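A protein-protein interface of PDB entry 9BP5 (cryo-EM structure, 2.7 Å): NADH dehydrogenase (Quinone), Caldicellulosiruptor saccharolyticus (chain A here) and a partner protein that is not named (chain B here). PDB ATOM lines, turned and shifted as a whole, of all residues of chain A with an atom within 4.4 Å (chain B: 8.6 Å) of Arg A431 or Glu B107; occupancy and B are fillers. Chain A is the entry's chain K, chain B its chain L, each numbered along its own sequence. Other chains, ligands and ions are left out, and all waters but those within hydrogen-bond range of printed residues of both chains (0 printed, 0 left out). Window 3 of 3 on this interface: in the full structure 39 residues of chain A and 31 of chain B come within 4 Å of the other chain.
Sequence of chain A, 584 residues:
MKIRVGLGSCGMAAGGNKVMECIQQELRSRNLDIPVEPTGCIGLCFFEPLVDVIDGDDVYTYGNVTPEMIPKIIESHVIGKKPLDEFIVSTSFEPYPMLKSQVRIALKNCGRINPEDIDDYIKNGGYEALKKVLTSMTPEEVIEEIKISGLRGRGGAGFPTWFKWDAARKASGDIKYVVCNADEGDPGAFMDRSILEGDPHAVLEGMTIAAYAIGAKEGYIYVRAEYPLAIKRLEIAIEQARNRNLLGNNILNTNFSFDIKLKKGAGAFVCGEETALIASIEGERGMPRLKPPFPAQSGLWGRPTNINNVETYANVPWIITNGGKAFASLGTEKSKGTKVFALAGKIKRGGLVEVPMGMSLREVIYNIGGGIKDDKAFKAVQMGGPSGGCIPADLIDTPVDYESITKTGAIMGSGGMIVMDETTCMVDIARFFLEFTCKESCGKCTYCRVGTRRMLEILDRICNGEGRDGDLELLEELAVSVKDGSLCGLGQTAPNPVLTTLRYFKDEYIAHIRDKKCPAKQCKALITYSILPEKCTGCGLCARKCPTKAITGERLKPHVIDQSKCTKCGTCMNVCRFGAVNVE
Of the printed residues of chain B, Ile A429 touches His B102 (3.8 Å) and Val B103 (3.8 Å). Leu A456 touches none of the printed residues of chain B. Printed residues of chain A within 4 Å of Gln B97: Phe A432 (3.3 Å). Printed residues of chain A within 4 Å of His B102: Asp A428, Ile A429, Arg A431 and Phe A432. Of the printed residues of chain A, Glu B107 touches Arg A431. The nearest printed residue of chain A that does not touch Gly B98 is Phe A433 (7.2 Å).
Of the 12 printed residues of chain A, 4 touch a printed residue of chain B. Hydrophobic or aromatic side chains of chain A that line the printed part of chain B: Ile A429 and Phe A432. Of the 23 printed residues of chain B, 5 touch a printed residue of chain A. Among the printed residues, 8 pairs touch across the chains.
Among the printed residues, pairs that only touch across the chains: Ile A429 with His B102 (3.8 Å), Ile A429 with Val B103 (3.8 Å), Arg A431 with His B102 (3.9 Å), Phe A432 with Gln B97 (3.3 Å), Phe A432 with Gly B98 (3.9 Å) and Phe A432 with His B102 (3.8 Å).
The side-chain carboxylate of Glu A435 lies within salt-bridge range of the guanidinium group of Arg A431 (3.2 Å). OE1 of Gln B95 lies within hydrogen-bond range of NE2 of Gln B97 (2.4 Å). SG of Cys B96 lies close to N of Gly B98. The side-chain amide nitrogen (NE2) of Gln B97 sits at hydrogen-bond distance from the side-chain hydroxyl (OG) of Ser B106 (3.0 Å). The backbone carbonyl oxygen of Glu B107 is in hydrogen-bond range of the side-chain amide nitrogen of Asn B111 (3.0 Å).
The side-chain carboxylate (OD2) of Asp A428 lies within hydrogen-bond range of a ring nitrogen (NE2) of His B102 (3.2 Å). NH2 of Arg A431 lies within salt-bridge range of OE2 of Glu B107, 3.4 Å away.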
ATOM      1  N   VAL A 427      -9.893  -7.776   2.946  1.00  0.00           N
ATOM      2  CA  VAL A 427      -9.630  -8.024   4.359  1.00  0.00           C
ATOM      3  C   VAL A 427      -8.942  -6.820   4.983  1.00  0.00           C
ATOM      4  O   VAL A 427      -9.213  -6.457   6.133  1.00  0.00           O
ATOM      5  CB  VAL A 427      -8.795  -9.304   4.528  1.00  0.00           C
ATOM      6  CG1 VAL A 427      -8.866  -9.793   5.950  1.00  0.00           C
ATOM      7  CG2 VAL A 427      -9.284 -10.371   3.580  1.00  0.00           C
ATOM      8  N   ASP A 428      -8.047  -6.179   4.231  1.00  0.00           N
ATOM      9  CA  ASP A 428      -7.365  -4.994   4.735  1.00  0.00           C
ATOM     10  C   ASP A 428      -8.341  -3.856   4.996  1.00  0.00           C
ATOM     11  O   ASP A 428      -8.240  -3.164   6.014  1.00  0.00           O
ATOM     12  CB  ASP A 428      -6.288  -4.557   3.749  1.00  0.00           C
ATOM     13  CG  ASP A 428      -5.503  -3.367   4.239  1.00  0.00           C
ATOM     14  OD1 ASP A 428      -5.024  -3.406   5.390  1.00  0.00           O
ATOM     15  OD2 ASP A 428      -5.361  -2.395   3.472  1.00  0.00           O
ATOM     16  N   ILE A 429      -9.294  -3.640   4.087  1.00  0.00           N
ATOM     17  CA  ILE A 429     -10.243  -2.548   4.275  1.00  0.00           C
ATOM     18  C   ILE A 429     -11.187  -2.853   5.433  1.00  0.00           C
ATOM     19  O   ILE A 429     -11.550  -1.956   6.207  1.00  0.00           O
ATOM     20  CB  ILE A 429     -10.991  -2.250   2.961  1.00  0.00           C
ATOM     21  CG1 ILE A 429     -11.135  -0.743   2.770  1.00  0.00           C
ATOM     22  CG2 ILE A 429     -12.362  -2.896   2.927  1.00  0.00           C
ATOM     23  CD1 ILE A 429      -9.850  -0.059   2.381  1.00  0.00           C
ATOM     24  N   ALA A 430     -11.582  -4.121   5.591  1.00  0.00           N
ATOM     25  CA  ALA A 430     -12.397  -4.488   6.744  1.00  0.00           C
ATOM     26  C   ALA A 430     -11.632  -4.259   8.039  1.00  0.00           C
ATOM     27  O   ALA A 430     -12.191  -3.759   9.024  1.00  0.00           O
ATOM     28  CB  ALA A 430     -12.846  -5.943   6.633  1.00  0.00           C
ATOM     29  N   ARG A 431     -10.344  -4.602   8.047  1.00  0.00           N
ATOM     30  CA  ARG A 431      -9.510  -4.348   9.213  1.00  0.00           C
ATOM     31  C   ARG A 431      -9.410  -2.859   9.504  1.00  0.00           C
ATOM     32  O   ARG A 431      -9.438  -2.446  10.667  1.00  0.00           O
ATOM     33  CB  ARG A 431      -8.122  -4.946   8.992  1.00  0.00           C
ATOM     34  CG  ARG A 431      -7.207  -4.862  10.184  1.00  0.00           C
ATOM     35  CD  ARG A 431      -5.818  -4.443   9.763  1.00  0.00           C
ATOM     36  NE  ARG A 431      -5.686  -2.992   9.734  1.00  0.00           N
ATOM     37  CZ  ARG A 431      -5.133  -2.309   8.742  1.00  0.00           C
ATOM     38  NH1 ARG A 431      -4.641  -2.916   7.675  1.00  0.00           N
ATOM     39  NH2 ARG A 431      -5.071  -0.983   8.823  1.00  0.00           N
ATOM     40  N   PHE A 432      -9.281  -2.037   8.462  1.00  0.00           N
ATOM     41  CA  PHE A 432      -9.184  -0.594   8.654  1.00  0.00           C
ATOM     42  C   PHE A 432     -10.461  -0.037   9.271  1.00  0.00           C
ATOM     43  O   PHE A 432     -10.417   0.763  10.217  1.00  0.00           O
ATOM     44  CB  PHE A 432      -8.883   0.080   7.316  1.00  0.00           C
ATOM     45  CG  PHE A 432      -9.232   1.540   7.269  1.00  0.00           C
ATOM     46  CD1 PHE A 432      -8.429   2.478   7.888  1.00  0.00           C
ATOM     47  CD2 PHE A 432     -10.350   1.975   6.584  1.00  0.00           C
ATOM     48  CE1 PHE A 432      -8.746   3.818   7.838  1.00  0.00           C
ATOM     49  CE2 PHE A 432     -10.671   3.311   6.532  1.00  0.00           C
ATOM     50  CZ  PHE A 432      -9.870   4.233   7.159  1.00  0.00           C
ATOM     51  N   PHE A 433     -11.614  -0.461   8.754  1.00  0.00           N
ATOM     52  CA  PHE A 433     -12.882   0.017   9.294  1.00  0.00           C
ATOM     53  C   PHE A 433     -13.072  -0.432  10.737  1.00  0.00           C
ATOM     54  O   PHE A 433     -13.543   0.341  11.581  1.00  0.00           O
ATOM     55  CB  PHE A 433     -14.036  -0.463   8.418  1.00  0.00           C
ATOM     56  CG  PHE A 433     -14.171   0.296   7.132  1.00  0.00           C
ATOM     57  CD1 PHE A 433     -14.389   1.658   7.140  1.00  0.00           C
ATOM     58  CD2 PHE A 433     -14.082  -0.352   5.918  1.00  0.00           C
ATOM     59  CE1 PHE A 433     -14.514   2.358   5.962  1.00  0.00           C
ATOM     60  CE2 PHE A 433     -14.205   0.345   4.740  1.00  0.00           C
ATOM     61  CZ  PHE A 433     -14.423   1.700   4.761  1.00  0.00           C
ATOM     62  N   LEU A 434     -12.699  -1.675  11.044  1.00  0.00           N
ATOM     63  CA  LEU A 434     -12.829  -2.160  12.414  1.00  0.00           C
ATOM     64  C   LEU A 434     -11.860  -1.453  13.351  1.00  0.00           C
ATOM     65  O   LEU A 434     -12.184  -1.216  14.517  1.00  0.00           O
ATOM     66  CB  LEU A 434     -12.610  -3.665  12.456  1.00  0.00           C
ATOM     67  CG  LEU A 434     -13.880  -4.482  12.279  1.00  0.00           C
ATOM     68  CD1 LEU A 434     -13.546  -5.927  12.475  1.00  0.00           C
ATOM     69  CD2 LEU A 434     -14.928  -4.038  13.272  1.00  0.00           C
ATOM     70  N   GLU A 435     -10.662  -1.121  12.867  1.00  0.00           N
ATOM     71  CA  GLU A 435      -9.726  -0.353  13.678  1.00  0.00           C
ATOM     72  C   GLU A 435     -10.289   1.022  13.999  1.00  0.00           C
ATOM     73  O   GLU A 435     -10.191   1.494  15.138  1.00  0.00           O
ATOM     74  CB  GLU A 435      -8.387  -0.227  12.954  1.00  0.00           C
ATOM     75  CG  GLU A 435      -7.198  -0.049  13.876  1.00  0.00           C
ATOM     76  CD  GLU A 435      -5.928  -0.653  13.311  1.00  0.00           C
ATOM     77  OE1 GLU A 435      -5.854  -0.837  12.078  1.00  0.00           O
ATOM     78  OE2 GLU A 435      -5.004  -0.943  14.098  1.00  0.00           O
ATOM     79  N   LEU A 456     -11.183  -7.167  15.535  1.00  0.00           N
ATOM     80  CA  LEU A 456      -9.963  -6.571  15.011  1.00  0.00           C
ATOM     81  C   LEU A 456      -8.773  -7.496  15.215  1.00  0.00           C
ATOM     82  O   LEU A 456      -7.885  -7.570  14.361  1.00  0.00           O
ATOM     83  CB  LEU A 456      -9.713  -5.219  15.672  1.00  0.00           C
ATOM     84  CG  LEU A 456      -8.478  -4.470  15.188  1.00  0.00           C
ATOM     85  CD1 LEU A 456      -8.670  -4.031  13.757  1.00  0.00           C
ATOM     86  CD2 LEU A 456      -8.192  -3.280  16.083  1.00  0.00           C
ATOM     87  N   LEU A 459      -8.973 -10.142  12.500  1.00  0.00           N
ATOM     88  CA  LEU A 459      -8.589  -9.607  11.198  1.00  0.00           C
ATOM     89  C   LEU A 459      -7.093  -9.331  11.130  1.00  0.00           C
ATOM     90  O   LEU A 459      -6.469  -9.530  10.083  1.00  0.00           O
ATOM     91  CB  LEU A 459      -9.388  -8.348  10.891  1.00  0.00           C
ATOM     92  CG  LEU A 459     -10.791  -8.622  10.359  1.00  0.00           C
ATOM     93  CD1 LEU A 459     -11.467  -7.336   9.968  1.00  0.00           C
ATOM     94  CD2 LEU A 459     -10.724  -9.560   9.181  1.00  0.00           C
ATOM     95  N   ASP A 460      -6.501  -8.869  12.232  1.00  0.00           N
ATOM     96  CA  ASP A 460      -5.056  -8.677  12.277  1.00  0.00           C
ATOM     97  C   ASP A 460      -4.324  -9.999  12.117  1.00  0.00           C
ATOM     98  O   ASP A 460      -3.309 -10.073  11.418  1.00  0.00           O
ATOM     99  CB  ASP A 460      -4.655  -8.005  13.588  1.00  0.00           C
ATOM    100  CG  ASP A 460      -4.875  -6.509  13.567  1.00  0.00           C
ATOM    101  OD1 ASP A 460      -5.571  -6.025  12.652  1.00  0.00           O
ATOM    102  OD2 ASP A 460      -4.350  -5.816  14.462  1.00  0.00           O
ATOM    103  N   GLN B  95      -1.646  13.540  10.089  1.00  0.00           N
ATOM    104  CA  GLN B  95      -1.575  12.608   8.971  1.00  0.00           C
ATOM    105  C   GLN B  95      -2.965  12.034   8.739  1.00  0.00           C
ATOM    106  O   GLN B  95      -3.451  11.224   9.536  1.00  0.00           O
ATOM    107  CB  GLN B  95      -0.559  11.506   9.257  1.00  0.00           C
ATOM    108  CG  GLN B  95       0.088  10.925   8.020  1.00  0.00           C
ATOM    109  CD  GLN B  95      -0.698   9.767   7.451  1.00  0.00           C
ATOM    110  OE1 GLN B  95      -1.147   8.888   8.185  1.00  0.00           O
ATOM    111  NE2 GLN B  95      -0.871   9.757   6.134  1.00  0.00           N
ATOM    112  N   CYS B  96      -3.610  12.458   7.655  1.00  0.00           N
ATOM    113  CA  CYS B  96      -4.965  12.010   7.373  1.00  0.00           C
ATOM    114  C   CYS B  96      -4.990  10.508   7.141  1.00  0.00           C
ATOM    115  O   CYS B  96      -4.140   9.962   6.434  1.00  0.00           O
ATOM    116  CB  CYS B  96      -5.521  12.743   6.155  1.00  0.00           C
ATOM    117  SG  CYS B  96      -7.168  12.205   5.666  1.00  0.00           S
ATOM    118  N   GLN B  97      -5.964   9.840   7.749  1.00  0.00           N
ATOM    119  CA  GLN B  97      -6.142   8.401   7.626  1.00  0.00           C
ATOM    120  C   GLN B  97      -7.588   8.067   7.304  1.00  0.00           C
ATOM    121  O   GLN B  97      -8.133   7.065   7.773  1.00  0.00           O
ATOM    122  CB  GLN B  97      -5.695   7.680   8.892  1.00  0.00           C
ATOM    123  CG  GLN B  97      -4.207   7.759   9.150  1.00  0.00           C
ATOM    124  CD  GLN B  97      -3.465   6.541   8.644  1.00  0.00           C
ATOM    125  OE1 GLN B  97      -3.937   5.413   8.775  1.00  0.00           O
ATOM    126  NE2 GLN B  97      -2.294   6.763   8.062  1.00  0.00           N
ATOM    127  N   GLY B  98      -8.232   8.901   6.500  1.00  0.00           N
ATOM    128  CA  GLY B  98      -9.572   8.616   6.045  1.00  0.00           C
ATOM    129  C   GLY B  98      -9.571   7.468   5.059  1.00  0.00           C
ATOM    130  O   GLY B  98      -8.535   6.913   4.692  1.00  0.00           O
ATOM    131  N   CYS B 101      -7.709   8.343   1.624  1.00  0.00           N
ATOM    132  CA  CYS B 101      -6.255   8.347   1.738  1.00  0.00           C
ATOM    133  C   CYS B 101      -5.715   6.942   1.968  1.00  0.00           C
ATOM    134  O   CYS B 101      -4.701   6.558   1.374  1.00  0.00           O
ATOM    135  CB  CYS B 101      -5.816   9.280   2.862  1.00  0.00           C
ATOM    136  SG  CYS B 101      -5.942  11.029   2.458  1.00  0.00           S
ATOM    137  N   HIS B 102      -6.378   6.160   2.821  1.00  0.00           N
ATOM    138  CA  HIS B 102      -5.910   4.805   3.088  1.00  0.00           C
ATOM    139  C   HIS B 102      -5.980   3.941   1.837  1.00  0.00           C
ATOM    140  O   HIS B 102      -5.086   3.124   1.588  1.00  0.00           O
ATOM    141  CB  HIS B 102      -6.721   4.177   4.217  1.00  0.00           C
ATOM    142  CG  HIS B 102      -6.369   2.749   4.487  1.00  0.00           C
ATOM    143  ND1 HIS B 102      -5.482   2.376   5.472  1.00  0.00           N
ATOM    144  CD2 HIS B 102      -6.784   1.601   3.901  1.00  0.00           C
ATOM    145  CE1 HIS B 102      -5.364   1.061   5.481  1.00  0.00           C
ATOM    146  NE2 HIS B 102      -6.143   0.567   4.537  1.00  0.00           N
ATOM    147  N   VAL B 103      -7.039   4.099   1.041  1.00  0.00           N
ATOM    148  CA  VAL B 103      -7.136   3.360  -0.214  1.00  0.00           C
ATOM    149  C   VAL B 103      -6.003   3.760  -1.151  1.00  0.00           C
ATOM    150  O   VAL B 103      -5.410   2.912  -1.829  1.00  0.00           O
ATOM    151  CB  VAL B 103      -8.518   3.577  -0.857  1.00  0.00           C
ATOM    152  CG1 VAL B 103      -8.469   3.292  -2.340  1.00  0.00           C
ATOM    153  CG2 VAL B 103      -9.547   2.689  -0.188  1.00  0.00           C
ATOM    154  N   ASN B 104      -5.670   5.049  -1.189  1.00  0.00           N
ATOM    155  CA  ASN B 104      -4.567   5.546  -2.001  1.00  0.00           C
ATOM    156  C   ASN B 104      -3.212   5.380  -1.328  1.00  0.00           C
ATOM    157  O   ASN B 104      -2.255   6.053  -1.721  1.00  0.00           O
ATOM    158  CB  ASN B 104      -4.794   7.015  -2.358  1.00  0.00           C
ATOM    159  CG  ASN B 104      -6.067   7.230  -3.143  1.00  0.00           C
ATOM    160  OD1 ASN B 104      -6.851   8.130  -2.848  1.00  0.00           O
ATOM    161  ND2 ASN B 104      -6.280   6.402  -4.157  1.00  0.00           N
ATOM    162  N   GLY B 105      -3.107   4.510  -0.329  1.00  0.00           N
ATOM    163  CA  GLY B 105      -1.828   4.217   0.285  1.00  0.00           C
ATOM    164  C   GLY B 105      -1.354   5.260   1.274  1.00  0.00           C
ATOM    165  O   GLY B 105      -0.315   5.890   1.065  1.00  0.00           O
ATOM    166  N   SER B 106      -2.106   5.453   2.357  1.00  0.00           N
ATOM    167  CA  SER B 106      -1.694   6.361   3.418  1.00  0.00           C
ATOM    168  C   SER B 106      -1.012   5.657   4.579  1.00  0.00           C
ATOM    169  O   SER B 106      -0.344   6.323   5.376  1.00  0.00           O
ATOM    170  CB  SER B 106      -2.897   7.139   3.956  1.00  0.00           C
ATOM    171  OG  SER B 106      -2.622   7.651   5.247  1.00  0.00           O
ATOM    172  N   GLU B 107      -1.170   4.337   4.701  1.00  0.00           N
ATOM    173  CA  GLU B 107      -0.498   3.611   5.772  1.00  0.00           C
ATOM    174  C   GLU B 107       1.014   3.688   5.620  1.00  0.00           C
ATOM    175  O   GLU B 107       1.739   3.844   6.610  1.00  0.00           O
ATOM    176  CB  GLU B 107      -0.960   2.156   5.789  1.00  0.00           C
ATOM    177  CG  GLU B 107      -1.597   1.728   7.095  1.00  0.00           C
ATOM    178  CD  GLU B 107      -1.948   0.255   7.113  1.00  0.00           C
ATOM    179  OE1 GLU B 107      -2.381  -0.266   6.064  1.00  0.00           O
ATOM    180  OE2 GLU B 107      -1.787  -0.383   8.175  1.00  0.00           O
ATOM    181  N   GLU B 108       1.508   3.576   4.386  1.00  0.00           N
ATOM    182  CA  GLU B 108       2.945   3.655   4.154  1.00  0.00           C
ATOM    183  C   GLU B 108       3.494   5.028   4.506  1.00  0.00           C
ATOM    184  O   GLU B 108       4.630   5.136   4.977  1.00  0.00           O
ATOM    185  CB  GLU B 108       3.262   3.308   2.701  1.00  0.00           C
ATOM    186  CG  GLU B 108       2.365   2.233   2.120  1.00  0.00           C
ATOM    187  CD  GLU B 108       2.520   0.901   2.825  1.00  0.00           C
ATOM    188  OE1 GLU B 108       3.610   0.639   3.375  1.00  0.00           O
ATOM    189  OE2 GLU B 108       1.551   0.113   2.829  1.00  0.00           O
ATOM    190  N   ILE B 109       2.708   6.085   4.297  1.00  0.00           N
ATOM    191  CA  ILE B 109       3.143   7.425   4.682  1.00  0.00           C
ATOM    192  C   ILE B 109       3.353   7.498   6.189  1.00  0.00           C
ATOM    193  O   ILE B 109       4.373   8.007   6.673  1.00  0.00           O
ATOM    194  CB  ILE B 109       2.123   8.473   4.207  1.00  0.00           C
ATOM    195  CG1 ILE B 109       1.625   8.131   2.804  1.00  0.00           C
ATOM    196  CG2 ILE B 109       2.723   9.862   4.246  1.00  0.00           C
ATOM    197  CD1 ILE B 109       2.596   8.483   1.714  1.00  0.00           C
ATOM    198  N   LYS B 110       2.387   6.985   6.954  1.00  0.00           N
ATOM    199  CA  LYS B 110       2.501   7.006   8.407  1.00  0.00           C
ATOM    200  C   LYS B 110       3.670   6.155   8.876  1.00  0.00           C
ATOM    201  O   LYS B 110       4.404   6.547   9.789  1.00  0.00           O
ATOM    202  CB  LYS B 110       1.199   6.525   9.043  1.00  0.00           C
ATOM    203  CG  LYS B 110       1.367   5.922  10.425  1.00  0.00           C
ATOM    204  CD  LYS B 110       0.046   5.399  10.962  1.00  0.00           C
ATOM    205  CE  LYS B 110      -0.207   3.972  10.510  1.00  0.00           C
ATOM    206  NZ  LYS B 110       0.884   3.056  10.935  1.00  0.00           N
ATOM    207  N   ASN B 111       3.858   4.984   8.266  1.00  0.00           N
ATOM    208  CA  ASN B 111       4.982   4.133   8.645  1.00  0.00           C
ATOM    209  C   ASN B 111       6.311   4.810   8.344  1.00  0.00           C
ATOM    210  O   ASN B 111       7.249   4.735   9.146  1.00  0.00           O
ATOM    211  CB  ASN B 111       4.887   2.788   7.929  1.00  0.00           C
ATOM    212  CG  ASN B 111       3.726   1.951   8.417  1.00  0.00           C
ATOM    213  OD1 ASN B 111       3.434   1.913   9.610  1.00  0.00           O
ATOM    214  ND2 ASN B 111       3.056   1.274   7.495  1.00  0.00           N
ATOM    215  N   ALA B 112       6.411   5.479   7.194  1.00  0.00           N
ATOM    216  CA  ALA B 112       7.640   6.184   6.853  1.00  0.00           C
ATOM    217  C   ALA B 112       7.919   7.309   7.838  1.00  0.00           C
ATOM    218  O   ALA B 112       9.061   7.489   8.275  1.00  0.00           O
ATOM    219  CB  ALA B 112       7.552   6.728   5.428  1.00  0.00           C
ATOM    220  N   LEU B 113       6.890   8.076   8.203  1.00  0.00           N
ATOM    221  CA  LEU B 113       7.093   9.151   9.170  1.00  0.00           C
ATOM    222  C   LEU B 113       7.484   8.603  10.537  1.00  0.00           C
ATOM    223  O   LEU B 113       8.347   9.170  11.216  1.00  0.00           O
ATOM    224  CB  LEU B 113       5.837  10.013   9.277  1.00  0.00           C
ATOM    225  CG  LEU B 113       5.396  10.747   8.012  1.00  0.00           C
ATOM    226  CD1 LEU B 113       4.320  11.763   8.338  1.00  0.00           C
ATOM    227  CD2 LEU B 113       6.580  11.413   7.344  1.00  0.00           C
ATOM    228  N   CYS B 114       6.857   7.502  10.960  1.00  0.00           N
ATOM    229  CA  CYS B 114       7.197   6.897  12.243  1.00  0.00           C
ATOM    230  C   CYS B 114       8.632   6.388  12.251  1.00  0.00           C
ATOM    231  O   CYS B 114       9.346   6.533  13.249  1.00  0.00           O
ATOM    232  CB  CYS B 114       6.225   5.761  12.562  1.00  0.00           C
ATOM    233  SG  CYS B 114       4.557   6.293  12.997  1.00  0.00           S
ATOM    234  N   ASP B 115       9.068   5.777  11.149  1.00  0.00           N
ATOM    235  CA  ASP B 115      10.440   5.290  11.072  1.00  0.00           C
ATOM    236  C   ASP B 115      11.434   6.443  11.022  1.00  0.00           C
ATOM    237  O   ASP B 115      12.524   6.354  11.596  1.00  0.00           O
ATOM    238  CB  ASP B 115      10.605   4.382   9.855  1.00  0.00           C
ATOM    239  CG  ASP B 115       9.786   3.111   9.963  1.00  0.00           C
ATOM    240  OD1 ASP B 115       9.393   2.749  11.092  1.00  0.00           O
ATOM    241  OD2 ASP B 115       9.534   2.474   8.918  1.00  0.00           O
ATOM    242  N   PRO B 121       2.716   6.593  16.515  1.00  0.00           N
ATOM    243  CA  PRO B 121       1.641   7.559  16.257  1.00  0.00           C
ATOM    244  C   PRO B 121       1.030   8.069  17.553  1.00  0.00           C
ATOM    245  O   PRO B 121       0.845   7.319  18.514  1.00  0.00           O
ATOM    246  CB  PRO B 121       0.628   6.752  15.440  1.00  0.00           C
ATOM    247  CG  PRO B 121       1.424   5.663  14.818  1.00  0.00           C
ATOM    248  CD  PRO B 121       2.491   5.318  15.812  1.00  0.00           C
ATOM    249  N   GLU B 134      -2.860  10.842  13.855  1.00  0.00           N
ATOM    250  CA  GLU B 134      -3.783  10.520  12.776  1.00  0.00           C
ATOM    251  C   GLU B 134      -5.081  11.299  12.941  1.00  0.00           C
ATOM    252  O   GLU B 134      -5.549  11.530  14.058  1.00  0.00           O
ATOM    253  CB  GLU B 134      -4.076   9.022  12.752  1.00  0.00           C
ATOM    254  CG  GLU B 134      -2.859   8.149  12.519  1.00  0.00           C
ATOM    255  CD  GLU B 134      -2.952   6.824  13.247  1.00  0.00           C
ATOM    256  OE1 GLU B 134      -4.083   6.390  13.548  1.00  0.00           O
ATOM    257  OE2 GLU B 134      -1.896   6.215  13.516  1.00  0.00           O
ATOM    258  N   PRO B 145      -2.546  10.668  -0.675  1.00  0.00           N
ATOM    259  CA  PRO B 145      -2.591  10.914   0.774  1.00  0.00           C
ATOM    260  C   PRO B 145      -2.230  12.349   1.139  1.00  0.00           C
ATOM    261  O   PRO B 145      -1.446  12.990   0.450  1.00  0.00           O
ATOM    262  CB  PRO B 145      -1.570   9.910   1.315  1.00  0.00           C
ATOM    263  CG  PRO B 145      -0.564   9.794   0.218  1.00  0.00           C
ATOM    264  CD  PRO B 145      -1.360   9.881  -1.056  1.00  0.00           C
ATOM    265  N   PRO B 159       5.981   7.582   0.383  1.00  0.00           N
ATOM    266  CA  PRO B 159       6.885   7.434   1.537  1.00  0.00           C
ATOM    267  C   PRO B 159       8.217   8.144   1.366  1.00  0.00           C
ATOM    268  O   PRO B 159       8.703   8.779   2.312  1.00  0.00           O
ATOM    269  CB  PRO B 159       7.062   5.915   1.638  1.00  0.00           C
ATOM    270  CG  PRO B 159       5.813   5.360   1.070  1.00  0.00           C
ATOM    271  CD  PRO B 159       5.386   6.296  -0.020  1.00  0.00           C
